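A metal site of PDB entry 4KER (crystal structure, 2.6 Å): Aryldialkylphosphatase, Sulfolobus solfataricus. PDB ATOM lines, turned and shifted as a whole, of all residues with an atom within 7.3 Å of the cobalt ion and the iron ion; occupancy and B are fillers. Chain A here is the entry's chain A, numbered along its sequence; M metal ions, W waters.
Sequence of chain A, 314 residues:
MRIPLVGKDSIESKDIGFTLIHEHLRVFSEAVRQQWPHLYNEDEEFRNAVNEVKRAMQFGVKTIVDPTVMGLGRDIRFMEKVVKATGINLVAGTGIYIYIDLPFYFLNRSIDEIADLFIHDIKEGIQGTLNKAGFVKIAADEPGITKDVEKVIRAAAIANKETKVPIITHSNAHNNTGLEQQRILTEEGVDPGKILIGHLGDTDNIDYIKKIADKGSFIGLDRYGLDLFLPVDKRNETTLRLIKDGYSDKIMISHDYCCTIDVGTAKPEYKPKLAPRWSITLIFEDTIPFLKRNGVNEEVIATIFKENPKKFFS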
ATOM      1  N   HIS A  22      24.151  13.771  -9.696  1.00  0.00           N
ATOM      2  CA  HIS A  22      23.278  12.741 -10.340  1.00  0.00           C
ATOM      3  C   HIS A  22      23.934  12.105 -11.552  1.00  0.00           C
ATOM      4  O   HIS A  22      23.769  12.599 -12.725  1.00  0.00           O
ATOM      5  CB  HIS A  22      21.936  13.347 -10.725  1.00  0.00           C
ATOM      6  CG  HIS A  22      20.861  12.303 -11.121  1.00  0.00           C
ATOM      7  ND1 HIS A  22      19.587  12.315 -10.620  1.00  0.00           N
ATOM      8  CD2 HIS A  22      20.920  11.191 -12.009  1.00  0.00           C
ATOM      9  CE1 HIS A  22      18.875  11.279 -11.148  1.00  0.00           C
ATOM     10  NE2 HIS A  22      19.691  10.594 -11.991  1.00  0.00           N
ATOM     11  N   GLU A  23      24.661  11.000 -11.314  1.00  0.00           N
ATOM     12  CA  GLU A  23      25.288  10.251 -12.393  1.00  0.00           C
ATOM     13  C   GLU A  23      25.103   8.739 -12.185  1.00  0.00           C
ATOM     14  O   GLU A  23      25.112   8.263 -11.057  1.00  0.00           O
ATOM     15  CB  GLU A  23      26.781  10.594 -12.511  1.00  0.00           C
ATOM     16  CG  GLU A  23      27.095  12.116 -12.603  1.00  0.00           C
ATOM     17  CD  GLU A  23      26.632  12.766 -13.965  1.00  0.00           C
ATOM     18  OE1 GLU A  23      26.559  14.020 -14.034  1.00  0.00           O
ATOM     19  OE2 GLU A  23      26.345  11.994 -14.944  1.00  0.00           O
ATOM     20  N   HIS A  24      24.930   7.996 -13.285  1.00  0.00           N
ATOM     21  CA  HIS A  24      24.759   6.526 -13.218  1.00  0.00           C
ATOM     22  C   HIS A  24      25.975   5.794 -13.788  1.00  0.00           C
ATOM     23  O   HIS A  24      26.337   6.003 -14.917  1.00  0.00           O
ATOM     24  CB  HIS A  24      23.489   6.082 -13.960  1.00  0.00           C
ATOM     25  CG  HIS A  24      22.211   6.709 -13.438  1.00  0.00           C
ATOM     26  ND1 HIS A  24      21.535   6.227 -12.366  1.00  0.00           N
ATOM     27  CD2 HIS A  24      21.476   7.819 -13.895  1.00  0.00           C
ATOM     28  CE1 HIS A  24      20.444   6.983 -12.138  1.00  0.00           C
ATOM     29  NE2 HIS A  24      20.398   7.952 -13.077  1.00  0.00           N
ATOM     30  N   VAL A  27      23.058   1.279 -15.771  1.00  0.00           N
ATOM     31  CA  VAL A  27      21.626   1.142 -15.604  1.00  0.00           C
ATOM     32  C   VAL A  27      21.080  -0.010 -16.449  1.00  0.00           C
ATOM     33  O   VAL A  27      21.426  -0.151 -17.629  1.00  0.00           O
ATOM     34  CB  VAL A  27      20.892   2.443 -15.992  1.00  0.00           C
ATOM     35  CG1 VAL A  27      19.393   2.195 -16.062  1.00  0.00           C
ATOM     36  CG2 VAL A  27      21.210   3.556 -15.008  1.00  0.00           C
ATOM     37  N   ASP A  66      25.459   8.482  -7.119  1.00  0.00           N
ATOM     38  CA  ASP A  66      24.824   7.589  -8.087  1.00  0.00           C
ATOM     39  C   ASP A  66      23.423   7.118  -7.603  1.00  0.00           C
ATOM     40  O   ASP A  66      23.322   6.297  -6.695  1.00  0.00           O
ATOM     41  CB  ASP A  66      25.733   6.362  -8.380  1.00  0.00           C
ATOM     42  CG  ASP A  66      25.195   5.471  -9.511  1.00  0.00           C
ATOM     43  OD1 ASP A  66      23.969   5.547  -9.820  1.00  0.00           O
ATOM     44  OD2 ASP A  66      26.005   4.700 -10.098  1.00  0.00           O
ATOM     45  N   PRO A  67      22.344   7.665  -8.230  1.00  0.00           N
ATOM     46  CA  PRO A  67      20.973   7.364  -7.842  1.00  0.00           C
ATOM     47  C   PRO A  67      20.407   6.074  -8.506  1.00  0.00           C
ATOM     48  O   PRO A  67      19.216   6.012  -8.798  1.00  0.00           O
ATOM     49  CB  PRO A  67      20.184   8.610  -8.342  1.00  0.00           C
ATOM     50  CG  PRO A  67      21.205   9.450  -9.116  1.00  0.00           C
ATOM     51  CD  PRO A  67      22.408   8.595  -9.339  1.00  0.00           C
ATOM     52  N   THR A  68      21.260   5.099  -8.741  1.00  0.00           N
ATOM     53  CA  THR A  68      20.830   3.816  -9.259  1.00  0.00           C
ATOM     54  C   THR A  68      20.259   2.942  -8.131  1.00  0.00           C
ATOM     55  O   THR A  68      20.967   2.634  -7.153  1.00  0.00           O
ATOM     56  CB  THR A  68      21.994   3.048  -9.949  1.00  0.00           C
ATOM     57  OG1 THR A  68      22.566   3.860 -10.974  1.00  0.00           O
ATOM     58  CG2 THR A  68      21.504   1.758 -10.564  1.00  0.00           C
ATOM     59  N   LEU A  72      16.464   0.165 -11.476  1.00  0.00           N
ATOM     60  CA  LEU A  72      17.529   0.669 -12.358  1.00  0.00           C
ATOM     61  C   LEU A  72      18.751  -0.252 -12.359  1.00  0.00           C
ATOM     62  O   LEU A  72      19.723  -0.019 -13.084  1.00  0.00           O
ATOM     63  CB  LEU A  72      17.929   2.082 -11.956  1.00  0.00           C
ATOM     64  CG  LEU A  72      16.865   3.175 -12.116  1.00  0.00           C
ATOM     65  CD1 LEU A  72      17.366   4.503 -11.533  1.00  0.00           C
ATOM     66  CD2 LEU A  72      16.450   3.342 -13.588  1.00  0.00           C
ATOM     67  N   TYR A  97      12.596   2.781  -7.701  1.00  0.00           N
ATOM     68  CA  TYR A  97      12.354   3.544  -8.894  1.00  0.00           C
ATOM     69  C   TYR A  97      11.207   2.937  -9.701  1.00  0.00           C
ATOM     70  O   TYR A  97      11.386   1.912 -10.354  1.00  0.00           O
ATOM     71  CB  TYR A  97      13.610   3.601  -9.749  1.00  0.00           C
ATOM     72  CG  TYR A  97      13.507   4.486 -10.947  1.00  0.00           C
ATOM     73  CD1 TYR A  97      12.837   4.045 -12.118  1.00  0.00           C
ATOM     74  CD2 TYR A  97      14.082   5.742 -10.950  1.00  0.00           C
ATOM     75  CE1 TYR A  97      12.746   4.850 -13.224  1.00  0.00           C
ATOM     76  CE2 TYR A  97      14.002   6.552 -12.063  1.00  0.00           C
ATOM     77  CZ  TYR A  97      13.328   6.115 -13.205  1.00  0.00           C
ATOM     78  OH  TYR A  97      13.254   6.923 -14.309  1.00  0.00           O
ATOM     79  N   TYR A  99       7.241   3.897 -12.014  1.00  0.00           N
ATOM     80  CA  TYR A  99       6.437   4.887 -12.686  1.00  0.00           C
ATOM     81  C   TYR A  99       4.960   4.688 -12.388  1.00  0.00           C
ATOM     82  O   TYR A  99       4.194   5.673 -12.263  1.00  0.00           O
ATOM     83  CB  TYR A  99       6.669   4.831 -14.194  1.00  0.00           C
ATOM     84  CG  TYR A  99       7.948   5.528 -14.657  1.00  0.00           C
ATOM     85  CD1 TYR A  99       9.037   5.743 -13.780  1.00  0.00           C
ATOM     86  CD2 TYR A  99       8.076   5.974 -15.982  1.00  0.00           C
ATOM     87  CE1 TYR A  99      10.199   6.364 -14.204  1.00  0.00           C
ATOM     88  CE2 TYR A  99       9.240   6.605 -16.428  1.00  0.00           C
ATOM     89  CZ  TYR A  99      10.296   6.802 -15.547  1.00  0.00           C
ATOM     90  OH  TYR A  99      11.431   7.425 -15.990  1.00  0.00           O
ATOM     91  N   KCX A 137      16.228   7.328  -3.009  1.00  0.00           N
ATOM     92  CA  KCX A 137      15.731   7.786  -4.338  1.00  0.00           C
ATOM     93  CB  KCX A 137      16.633   7.235  -5.474  1.00  0.00           C
ATOM     94  CG  KCX A 137      16.759   8.266  -6.643  1.00  0.00           C
ATOM     95  CD  KCX A 137      15.706   8.037  -7.700  1.00  0.00           C
ATOM     96  CE  KCX A 137      15.914   8.960  -8.920  1.00  0.00           C
ATOM     97  NZ  KCX A 137      16.910   8.429  -9.846  1.00  0.00           N
ATOM     98  C   KCX A 137      14.318   7.344  -4.577  1.00  0.00           C
ATOM     99  O   KCX A 137      13.959   6.231  -4.264  1.00  0.00           O
ATOM    100  CX  KCX A 137      17.024   8.840 -11.110  1.00  0.00           C
ATOM    101  OQ1 KCX A 137      17.961   8.289 -11.863  1.00  0.00           O
ATOM    102  OQ2 KCX A 137      16.292   9.713 -11.616  1.00  0.00           O
ATOM    103  N   ILE A 138      13.528   8.221  -5.130  1.00  0.00           N
ATOM    104  CA  ILE A 138      12.160   7.909  -5.472  1.00  0.00           C
ATOM    105  C   ILE A 138      11.823   8.579  -6.786  1.00  0.00           C
ATOM    106  O   ILE A 138      12.551   9.475  -7.229  1.00  0.00           O
ATOM    107  CB  ILE A 138      11.166   8.358  -4.354  1.00  0.00           C
ATOM    108  CG1 ILE A 138      11.268   9.875  -4.107  1.00  0.00           C
ATOM    109  CG2 ILE A 138      11.431   7.589  -3.069  1.00  0.00           C
ATOM    110  CD1 ILE A 138      10.493  10.715  -5.094  1.00  0.00           C
ATOM    111  N   ALA A 139      10.725   8.145  -7.425  1.00  0.00           N
ATOM    112  CA  ALA A 139      10.430   8.649  -8.768  1.00  0.00           C
ATOM    113  C   ALA A 139       8.948   8.781  -9.101  1.00  0.00           C
ATOM    114  O   ALA A 139       8.070   8.234  -8.412  1.00  0.00           O
ATOM    115  CB  ALA A 139      11.120   7.783  -9.806  1.00  0.00           C
ATOM    116  N   ASP A 141       6.696   9.967 -13.013  1.00  0.00           N
ATOM    117  CA  ASP A 141       6.836  10.473 -14.365  1.00  0.00           C
ATOM    118  C   ASP A 141       5.469  10.767 -15.025  1.00  0.00           C
ATOM    119  O   ASP A 141       4.530  11.182 -14.364  1.00  0.00           O
ATOM    120  CB  ASP A 141       7.654   9.497 -15.221  1.00  0.00           C
ATOM    121  CG  ASP A 141       8.453  10.208 -16.322  1.00  0.00           C
ATOM    122  OD1 ASP A 141       7.840  10.646 -17.337  1.00  0.00           O
ATOM    123  OD2 ASP A 141       9.701  10.313 -16.185  1.00  0.00           O
ATOM    124  N   THR A 169      14.962  12.863  -6.109  1.00  0.00           N
ATOM    125  CA  THR A 169      13.779  12.376  -6.866  1.00  0.00           C
ATOM    126  C   THR A 169      13.961  12.434  -8.340  1.00  0.00           C
ATOM    127  O   THR A 169      14.711  13.239  -8.854  1.00  0.00           O
ATOM    128  CB  THR A 169      12.480  13.184  -6.502  1.00  0.00           C
ATOM    129  OG1 THR A 169      12.413  14.391  -7.287  1.00  0.00           O
ATOM    130  CG2 THR A 169      12.452  13.530  -5.009  1.00  0.00           C
ATOM    131  N   HIS A 170      13.270  11.570  -9.018  1.00  0.00           N
ATOM    132  CA  HIS A 170      13.126  11.632 -10.428  1.00  0.00           C
ATOM    133  C   HIS A 170      11.767  12.130 -10.685  1.00  0.00           C
ATOM    134  O   HIS A 170      10.781  11.631 -10.087  1.00  0.00           O
ATOM    135  CB  HIS A 170      13.289  10.229 -11.019  1.00  0.00           C
ATOM    136  CG  HIS A 170      12.920  10.141 -12.486  1.00  0.00           C
ATOM    137  ND1 HIS A 170      13.854  10.003 -13.481  1.00  0.00           N
ATOM    138  CD2 HIS A 170      11.663  10.161 -13.134  1.00  0.00           C
ATOM    139  CE1 HIS A 170      13.231   9.939 -14.671  1.00  0.00           C
ATOM    140  NE2 HIS A 170      11.889  10.049 -14.462  1.00  0.00           N
ATOM    141  N   SER A 171      11.656  13.133 -11.553  1.00  0.00           N
ATOM    142  CA  SER A 171      10.290  13.697 -11.886  1.00  0.00           C
ATOM    143  C   SER A 171      10.168  14.135 -13.348  1.00  0.00           C
ATOM    144  O   SER A 171      11.154  14.251 -14.063  1.00  0.00           O
ATOM    145  CB  SER A 171       9.938  14.874 -10.951  1.00  0.00           C
ATOM    146  OG  SER A 171      10.514  16.087 -11.405  1.00  0.00           O
ATOM    147  N   GLY A 198      14.363  16.392  -8.894  1.00  0.00           N
ATOM    148  CA  GLY A 198      15.196  16.139 -10.059  1.00  0.00           C
ATOM    149  C   GLY A 198      14.562  16.405 -11.424  1.00  0.00           C
ATOM    150  O   GLY A 198      13.345  16.429 -11.572  1.00  0.00           O
ATOM    151  N   HIS A 199      15.444  16.614 -12.423  1.00  0.00           N
ATOM    152  CA  HIS A 199      15.032  16.737 -13.860  1.00  0.00           C
ATOM    153  C   HIS A 199      14.230  17.964 -14.178  1.00  0.00           C
ATOM    154  O   HIS A 199      13.497  18.006 -15.170  1.00  0.00           O
ATOM    155  CB  HIS A 199      14.303  15.468 -14.339  1.00  0.00           C
ATOM    156  CG  HIS A 199      15.044  14.172 -14.001  1.00  0.00           C
ATOM    157  ND1 HIS A 199      16.409  14.083 -13.969  1.00  0.00           N
ATOM    158  CD2 HIS A 199      14.564  12.883 -13.694  1.00  0.00           C
ATOM    159  CE1 HIS A 199      16.775  12.811 -13.651  1.00  0.00           C
ATOM    160  NE2 HIS A 199      15.649  12.082 -13.489  1.00  0.00           N
ATOM    161  N   ASP A 222      19.763  18.620 -14.026  1.00  0.00           N
ATOM    162  CA  ASP A 222      20.649  17.487 -13.937  1.00  0.00           C
ATOM    163  C   ASP A 222      20.651  16.565 -15.185  1.00  0.00           C
ATOM    164  O   ASP A 222      21.033  15.396 -15.101  1.00  0.00           O
ATOM    165  CB  ASP A 222      20.273  16.657 -12.701  1.00  0.00           C
ATOM    166  CG  ASP A 222      18.746  16.305 -12.660  1.00  0.00           C
ATOM    167  OD1 ASP A 222      18.211  16.079 -11.539  1.00  0.00           O
ATOM    168  OD2 ASP A 222      18.116  16.282 -13.741  1.00  0.00           O
ATOM    169  N   ARG A 223      20.249  17.085 -16.317  1.00  0.00           N
ATOM    170  CA  ARG A 223      20.259  16.270 -17.556  1.00  0.00           C
ATOM    171  C   ARG A 223      20.974  16.962 -18.742  1.00  0.00           C
ATOM    172  O   ARG A 223      20.561  16.820 -19.899  1.00  0.00           O
ATOM    173  CB  ARG A 223      18.850  15.820 -17.931  1.00  0.00           C
ATOM    174  CG  ARG A 223      18.332  14.652 -17.096  1.00  0.00           C
ATOM    175  CD  ARG A 223      16.948  14.198 -17.545  1.00  0.00           C
ATOM    176  NE  ARG A 223      16.614  12.884 -16.999  1.00  0.00           N
ATOM    177  CZ  ARG A 223      15.429  12.292 -17.148  1.00  0.00           C
ATOM    178  NH1 ARG A 223      14.445  12.891 -17.808  1.00  0.00           N
ATOM    179  NH2 ARG A 223      15.221  11.072 -16.606  1.00  0.00           N
ATOM    180  N   HIS A 255      24.555  15.546 -15.120  1.00  0.00           N
ATOM    181  CA  HIS A 255      24.292  15.023 -16.482  1.00  0.00           C
ATOM    182  C   HIS A 255      23.239  13.928 -16.535  1.00  0.00           C
ATOM    183  O   HIS A 255      22.567  13.751 -17.545  1.00  0.00           O
ATOM    184  CB  HIS A 255      25.593  14.502 -17.123  1.00  0.00           C
ATOM    185  CG  HIS A 255      26.709  15.530 -17.159  1.00  0.00           C
ATOM    186  ND1 HIS A 255      27.700  15.561 -16.232  1.00  0.00           N
ATOM    187  CD2 HIS A 255      26.978  16.582 -18.052  1.00  0.00           C
ATOM    188  CE1 HIS A 255      28.544  16.564 -16.516  1.00  0.00           C
ATOM    189  NE2 HIS A 255      28.106  17.192 -17.625  1.00  0.00           N
ATOM    190  N   ASP A 256      23.108  13.173 -15.439  1.00  0.00           N
ATOM    191  CA  ASP A 256      22.266  11.957 -15.446  1.00  0.00           C
ATOM    192  C   ASP A 256      22.803  11.007 -16.507  1.00  0.00           C
ATOM    193  O   ASP A 256      22.061  10.227 -17.110  1.00  0.00           O
ATOM    194  CB  ASP A 256      20.816  12.308 -15.744  1.00  0.00           C
ATOM    195  CG  ASP A 256      19.803  11.076 -15.438  1.00  0.00           C
ATOM    196  OD1 ASP A 256      20.099  10.198 -14.496  1.00  0.00           O
ATOM    197  OD2 ASP A 256      18.748  10.997 -16.124  1.00  0.00           O
ATOM    198  N   TYR A 257      24.110  11.068 -16.737  1.00  0.00           N
ATOM    199  CA  TYR A 257      24.718  10.275 -17.756  1.00  0.00           C
ATOM    200  C   TYR A 257      24.805   8.818 -17.377  1.00  0.00           C
ATOM    201  O   TYR A 257      25.157   8.467 -16.232  1.00  0.00           O
ATOM    202  CB  TYR A 257      26.131  10.814 -18.088  1.00  0.00           C
ATOM    203  CG  TYR A 257      26.815  10.038 -19.160  1.00  0.00           C
ATOM    204  CD1 TYR A 257      27.786   9.085 -18.840  1.00  0.00           C
ATOM    205  CD2 TYR A 257      26.506  10.237 -20.509  1.00  0.00           C
ATOM    206  CE1 TYR A 257      28.424   8.357 -19.826  1.00  0.00           C
ATOM    207  CE2 TYR A 257      27.134   9.513 -21.512  1.00  0.00           C
ATOM    208  CZ  TYR A 257      28.092   8.579 -21.168  1.00  0.00           C
ATOM    209  OH  TYR A 257      28.725   7.853 -22.162  1.00  0.00           O
ATOM    210  N   CYS A 258      24.477   7.956 -18.329  1.00  0.00           N
ATOM    211  CA  CYS A 258      24.585   6.547 -18.141  1.00  0.00           C
ATOM    212  C   CYS A 258      25.756   6.027 -18.906  1.00  0.00           C
ATOM    213  O   CYS A 258      25.709   5.917 -20.153  1.00  0.00           O
ATOM    214  CB  CYS A 258      23.298   5.845 -18.613  1.00  0.00           C
ATOM    215  SG  CYS A 258      21.809   6.387 -17.784  1.00  0.00           S
HETATM  216 CO    CO M   1      15.777  10.175 -13.290  1.00  0.00          CO
HETATM  217 FE    FE M   2      18.962   9.268 -13.245  1.00  0.00          FE
HETATM  218  O   HOH W   1      17.298   9.491 -14.471  1.00  0.00           O
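Water W1 bridges the side-chain carboxylate (OD2) of Asp 256 (2.7 Å) and the guanidinium group (NH2) of Arg 223 (3.4 Å).
OQ2 of KCX 137 is bound to the cobalt ion, 1.8 Å away.
NE2 of His 199 binds the cobalt ion (1.9 Å).
The cobalt ion is bound by ND1 of His 170 (1.9 Å).
The cobalt ion is bound by water W1 (2.0 Å).
The cobalt ion has four donor atoms within binding distance.
The iron ion is bound by OD1 of Asp 256 (1.9 Å).
The iron ion is bound by NE2 of His 24, 2.0 Å away.
NE2 of His 22 binds the iron ion, at 2.0 Å.
OQ1 of KCX 137 binds the iron ion, at 2.0 Å.
Water W1 is bound to the iron ion (2.1 Å).
Merely in contact with the cobalt ion: Arg 223 (3.5 Å).
Of the 25 residues printed, 5 come within 4 Å of the cobalt ion.
The guanidinium group of Arg 223 lies within hydrogen-bond range of a ring nitrogen (ND1) of His 199 (3.3 Å).
The side-chain carboxylate (OD2) of Asp 222 lies within hydrogen-bond range of a ring nitrogen (ND1) of His 199, 2.8 Å away.
The guanidinium group of Arg 223 lies within salt-bridge range of the side-chain carboxylate of Asp 256, 3.0 Å away.
The backbone NH (N) of Asp 256 sits at hydrogen-bond distance from the side-chain carboxylate (OE2) of Glu 23.
N of Asp 256 sits at hydrogen-bond distance from O of Asp 222, 3.1 Å away.
NE2 of His 170 sits close to OH of Tyr 97, 3.4 Å away.
A ring nitrogen (NE2) of His 170 is in hydrogen-bond range of the side-chain carboxylate of Asp 141 (2.8 Å).
ND1 of His 24 is in hydrogen-bond range of OG1 of Thr 68 (2.9 Å).
The nearest printed residue that does not touch the iron ion is His 199 (4.2 Å).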
